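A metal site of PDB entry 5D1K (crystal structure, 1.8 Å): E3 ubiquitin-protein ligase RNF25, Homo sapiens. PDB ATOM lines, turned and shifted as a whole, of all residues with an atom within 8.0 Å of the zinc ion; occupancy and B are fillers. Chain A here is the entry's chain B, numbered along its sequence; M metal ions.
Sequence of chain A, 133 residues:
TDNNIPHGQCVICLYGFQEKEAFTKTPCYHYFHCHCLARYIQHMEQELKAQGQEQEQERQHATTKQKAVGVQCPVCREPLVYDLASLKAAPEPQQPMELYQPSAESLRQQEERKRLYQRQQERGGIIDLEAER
Within 4 Å of the zinc ion: Cys 28, His 30, Cys 73 and Cys 76.
SG of Cys 76 sits close to N of Glu 78 (3.7 Å).
SG of Cys 73 sits close to N of Val 75 (3.4 Å).
The side-chain hydroxyl of Thr 26 sits at hydrogen-bond distance from the backbone NH of His 30, 3.1 Å away.
N of Cys 73 is in hydrogen-bond range of O of Glu 78.
N of Cys 28 lies close to OG1 of Thr 26, at 3.4 Å.
The zinc ion is bound by a ring nitrogen (ND1) of His 30 (2.0 Å), the side-chain sulfur of Cys 73 (2.3 Å), the side-chain sulfur of Cys 28 (2.3 Å) and the side-chain sulfur of Cys 76 (2.4 Å).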
ATOM      1  N   THR A  26      -8.085 -24.102  25.084  1.00  0.00           N
ATOM      2  CA  THR A  26      -7.159 -25.195  24.783  1.00  0.00           C
ATOM      3  C   THR A  26      -7.025 -25.396  23.264  1.00  0.00           C
ATOM      4  O   THR A  26      -7.830 -24.876  22.500  1.00  0.00           O
ATOM      5  CB  THR A  26      -7.664 -26.498  25.367  1.00  0.00           C
ATOM      6  OG1 THR A  26      -8.911 -26.807  24.771  1.00  0.00           O
ATOM      7  CG2 THR A  26      -7.844 -26.372  26.883  1.00  0.00           C
ATOM      8  N   PRO A  27      -6.001 -26.161  22.825  1.00  0.00           N
ATOM      9  CA  PRO A  27      -5.885 -26.429  21.379  1.00  0.00           C
ATOM     10  C   PRO A  27      -7.007 -27.326  20.888  1.00  0.00           C
ATOM     11  O   PRO A  27      -7.143 -27.487  19.671  1.00  0.00           O
ATOM     12  CB  PRO A  27      -4.525 -27.140  21.266  1.00  0.00           C
ATOM     13  CG  PRO A  27      -3.770 -26.686  22.539  1.00  0.00           C
ATOM     14  CD  PRO A  27      -4.846 -26.676  23.580  1.00  0.00           C
ATOM     15  N   CYS A  28      -7.787 -27.897  21.800  1.00  0.00           N
ATOM     16  CA  CYS A  28      -8.969 -28.673  21.452  1.00  0.00           C
ATOM     17  C   CYS A  28     -10.267 -27.877  21.534  1.00  0.00           C
ATOM     18  O   CYS A  28     -11.352 -28.458  21.543  1.00  0.00           O
ATOM     19  CB  CYS A  28      -9.046 -29.963  22.284  1.00  0.00           C
ATOM     20  SG  CYS A  28      -8.851 -29.726  24.092  1.00  0.00           S
ATOM     21  N   TYR A  29     -10.132 -26.544  21.624  1.00  0.00           N
ATOM     22  CA  TYR A  29     -11.226 -25.581  21.436  1.00  0.00           C
ATOM     23  C   TYR A  29     -12.174 -25.496  22.612  1.00  0.00           C
ATOM     24  O   TYR A  29     -13.340 -25.154  22.448  1.00  0.00           O
ATOM     25  CB  TYR A  29     -12.015 -25.849  20.139  1.00  0.00           C
ATOM     26  CG  TYR A  29     -11.099 -26.130  18.965  1.00  0.00           C
ATOM     27  CD1 TYR A  29     -10.341 -25.114  18.397  1.00  0.00           C
ATOM     28  CD2 TYR A  29     -11.004 -27.408  18.440  1.00  0.00           C
ATOM     29  CE1 TYR A  29      -9.493 -25.376  17.318  1.00  0.00           C
ATOM     30  CE2 TYR A  29     -10.154 -27.680  17.363  1.00  0.00           C
ATOM     31  CZ  TYR A  29      -9.409 -26.665  16.813  1.00  0.00           C
ATOM     32  OH  TYR A  29      -8.591 -26.934  15.739  1.00  0.00           O
ATOM     33  N   HIS A  30     -11.644 -25.782  23.798  1.00  0.00           N
ATOM     34  CA  HIS A  30     -12.439 -25.735  25.015  1.00  0.00           C
ATOM     35  C   HIS A  30     -11.959 -24.632  25.941  1.00  0.00           C
ATOM     36  O   HIS A  30     -10.761 -24.445  26.102  1.00  0.00           O
ATOM     37  CB  HIS A  30     -12.421 -27.111  25.676  1.00  0.00           C
ATOM     38  CG  HIS A  30     -13.077 -28.152  24.828  1.00  0.00           C
ATOM     39  ND1 HIS A  30     -12.458 -29.334  24.460  1.00  0.00           N
ATOM     40  CD2 HIS A  30     -14.302 -28.161  24.242  1.00  0.00           C
ATOM     41  CE1 HIS A  30     -13.276 -30.020  23.683  1.00  0.00           C
ATOM     42  NE2 HIS A  30     -14.399 -29.339  23.541  1.00  0.00           N
ATOM     43  N   TYR A  31     -12.913 -23.908  26.541  1.00  0.00           N
ATOM     44  CA  TYR A  31     -12.579 -22.745  27.360  1.00  0.00           C
ATOM     45  C   TYR A  31     -12.726 -23.044  28.842  1.00  0.00           C
ATOM     46  O   TYR A  31     -13.706 -23.671  29.248  1.00  0.00           O
ATOM     47  CB  TYR A  31     -13.502 -21.573  27.021  1.00  0.00           C
ATOM     48  CG  TYR A  31     -13.255 -20.947  25.663  1.00  0.00           C
ATOM     49  CD1 TYR A  31     -13.908 -21.427  24.532  1.00  0.00           C
ATOM     50  CD2 TYR A  31     -12.388 -19.870  25.517  1.00  0.00           C
ATOM     51  CE1 TYR A  31     -13.687 -20.853  23.281  1.00  0.00           C
ATOM     52  CE2 TYR A  31     -12.166 -19.296  24.266  1.00  0.00           C
ATOM     53  CZ  TYR A  31     -12.823 -19.793  23.165  1.00  0.00           C
ATOM     54  OH  TYR A  31     -12.623 -19.225  21.915  1.00  0.00           O
ATOM     55  N   PHE A  32     -11.766 -22.550  29.627  1.00  0.00           N
ATOM     56  CA  PHE A  32     -11.827 -22.683  31.089  1.00  0.00           C
ATOM     57  C   PHE A  32     -11.320 -21.402  31.713  1.00  0.00           C
ATOM     58  O   PHE A  32     -10.490 -20.726  31.125  1.00  0.00           O
ATOM     59  CB  PHE A  32     -10.951 -23.836  31.561  1.00  0.00           C
ATOM     60  CG  PHE A  32     -11.255 -25.155  30.897  1.00  0.00           C
ATOM     61  CD1 PHE A  32     -12.214 -26.021  31.417  1.00  0.00           C
ATOM     62  CD2 PHE A  32     -10.557 -25.539  29.753  1.00  0.00           C
ATOM     63  CE1 PHE A  32     -12.476 -27.228  30.804  1.00  0.00           C
ATOM     64  CE2 PHE A  32     -10.817 -26.756  29.142  1.00  0.00           C
ATOM     65  CZ  PHE A  32     -11.777 -27.600  29.667  1.00  0.00           C
ATOM     66  N   GLN A  72      -5.134 -34.675  30.721  1.00  0.00           N
ATOM     67  CA  GLN A  72      -6.044 -34.597  29.569  1.00  0.00           C
ATOM     68  C   GLN A  72      -7.088 -33.519  29.771  1.00  0.00           C
ATOM     69  O   GLN A  72      -7.437 -33.182  30.909  1.00  0.00           O
ATOM     70  CB  GLN A  72      -6.750 -35.945  29.392  1.00  0.00           C
ATOM     71  CG  GLN A  72      -5.825 -37.081  29.012  1.00  0.00           C
ATOM     72  CD  GLN A  72      -6.474 -38.434  29.176  1.00  0.00           C
ATOM     73  OE1 GLN A  72      -7.529 -38.567  29.800  1.00  0.00           O
ATOM     74  NE2 GLN A  72      -5.858 -39.462  28.594  1.00  0.00           N
ATOM     75  N   CYS A  73      -7.606 -32.966  28.676  1.00  0.00           N
ATOM     76  CA  CYS A  73      -8.733 -32.046  28.733  1.00  0.00           C
ATOM     77  C   CYS A  73      -9.905 -32.709  29.436  1.00  0.00           C
ATOM     78  O   CYS A  73     -10.291 -33.821  29.096  1.00  0.00           O
ATOM     79  CB  CYS A  73      -9.213 -31.689  27.319  1.00  0.00           C
ATOM     80  SG  CYS A  73     -10.596 -30.572  27.261  1.00  0.00           S
ATOM     81  N   PRO A  74     -10.493 -32.009  30.416  1.00  0.00           N
ATOM     82  CA  PRO A  74     -11.633 -32.575  31.146  1.00  0.00           C
ATOM     83  C   PRO A  74     -12.836 -32.849  30.233  1.00  0.00           C
ATOM     84  O   PRO A  74     -13.647 -33.717  30.557  1.00  0.00           O
ATOM     85  CB  PRO A  74     -12.009 -31.455  32.124  1.00  0.00           C
ATOM     86  CG  PRO A  74     -10.847 -30.587  32.227  1.00  0.00           C
ATOM     87  CD  PRO A  74     -10.056 -30.716  30.955  1.00  0.00           C
ATOM     88  N   VAL A  75     -12.931 -32.126  29.127  1.00  0.00           N
ATOM     89  CA  VAL A  75     -14.081 -32.258  28.231  1.00  0.00           C
ATOM     90  C   VAL A  75     -13.938 -33.409  27.235  1.00  0.00           C
ATOM     91  O   VAL A  75     -14.843 -34.239  27.090  1.00  0.00           O
ATOM     92  CB  VAL A  75     -14.357 -30.932  27.479  1.00  0.00           C
ATOM     93  CG1 VAL A  75     -15.415 -31.122  26.393  1.00  0.00           C
ATOM     94  CG2 VAL A  75     -14.806 -29.873  28.452  1.00  0.00           C
ATOM     95  N   CYS A  76     -12.783 -33.478  26.561  1.00  0.00           N
ATOM     96  CA  CYS A  76     -12.653 -34.356  25.393  1.00  0.00           C
ATOM     97  C   CYS A  76     -11.460 -35.300  25.472  1.00  0.00           C
ATOM     98  O   CYS A  76     -11.220 -36.082  24.544  1.00  0.00           O
ATOM     99  CB  CYS A  76     -12.557 -33.505  24.126  1.00  0.00           C
ATOM    100  SG  CYS A  76     -10.985 -32.626  23.948  1.00  0.00           S
ATOM    101  N   ARG A  77     -10.720 -35.222  26.570  1.00  0.00           N
ATOM    102  CA  ARG A  77      -9.602 -36.108  26.874  1.00  0.00           C
ATOM    103  C   ARG A  77      -8.357 -35.913  26.003  1.00  0.00           C
ATOM    104  O   ARG A  77      -7.402 -36.685  26.102  1.00  0.00           O
ATOM    105  CB  ARG A  77     -10.032 -37.580  26.851  1.00  0.00           C
ATOM    106  CG  ARG A  77     -11.023 -37.939  27.931  1.00  0.00           C
ATOM    107  CD  ARG A  77     -11.305 -39.426  27.967  1.00  0.00           C
ATOM    108  NE  ARG A  77     -12.351 -39.722  28.942  1.00  0.00           N
ATOM    109  CZ  ARG A  77     -12.148 -39.801  30.250  1.00  0.00           C
ATOM    110  NH1 ARG A  77     -10.934 -39.610  30.745  1.00  0.00           N
ATOM    111  NH2 ARG A  77     -13.158 -40.070  31.063  1.00  0.00           N
ATOM    112  N   GLU A  78      -8.337 -34.891  25.148  1.00  0.00           N
ATOM    113  CA  GLU A  78      -7.116 -34.608  24.412  1.00  0.00           C
ATOM    114  C   GLU A  78      -6.030 -34.176  25.394  1.00  0.00           C
ATOM    115  O   GLU A  78      -6.298 -33.411  26.328  1.00  0.00           O
ATOM    116  CB  GLU A  78      -7.320 -33.520  23.349  1.00  0.00           C
ATOM    117  CG  GLU A  78      -6.016 -33.066  22.698  1.00  0.00           C
ATOM    118  CD  GLU A  78      -6.219 -32.179  21.484  1.00  0.00           C
ATOM    119  OE1 GLU A  78      -7.047 -32.528  20.606  1.00  0.00           O
ATOM    120  OE2 GLU A  78      -5.529 -31.141  21.378  1.00  0.00           O
ATOM    121  N   PRO A  79      -4.805 -34.691  25.223  1.00  0.00           N
ATOM    122  CA  PRO A  79      -3.728 -34.283  26.136  1.00  0.00           C
ATOM    123  C   PRO A  79      -3.475 -32.776  26.074  1.00  0.00           C
ATOM    124  O   PRO A  79      -3.370 -32.218  24.987  1.00  0.00           O
ATOM    125  CB  PRO A  79      -2.520 -35.056  25.610  1.00  0.00           C
ATOM    126  CG  PRO A  79      -3.094 -36.241  24.912  1.00  0.00           C
ATOM    127  CD  PRO A  79      -4.370 -35.747  24.290  1.00  0.00           C
ATOM    128  N   LEU A  80      -3.369 -32.121  27.225  1.00  0.00           N
ATOM    129  CA  LEU A  80      -3.235 -30.664  27.246  1.00  0.00           C
ATOM    130  C   LEU A  80      -1.781 -30.217  27.177  1.00  0.00           C
ATOM    131  O   LEU A  80      -0.910 -30.887  27.734  1.00  0.00           O
ATOM    132  CB  LEU A  80      -3.848 -30.112  28.520  1.00  0.00           C
ATOM    133  CG  LEU A  80      -5.372 -30.122  28.558  1.00  0.00           C
ATOM    134  CD1 LEU A  80      -5.822 -29.342  29.759  1.00  0.00           C
ATOM    135  CD2 LEU A  80      -5.939 -29.517  27.278  1.00  0.00           C
HETATM  136 ZN    ZN M   1     -10.851 -30.488  24.992  1.00  0.00          ZN
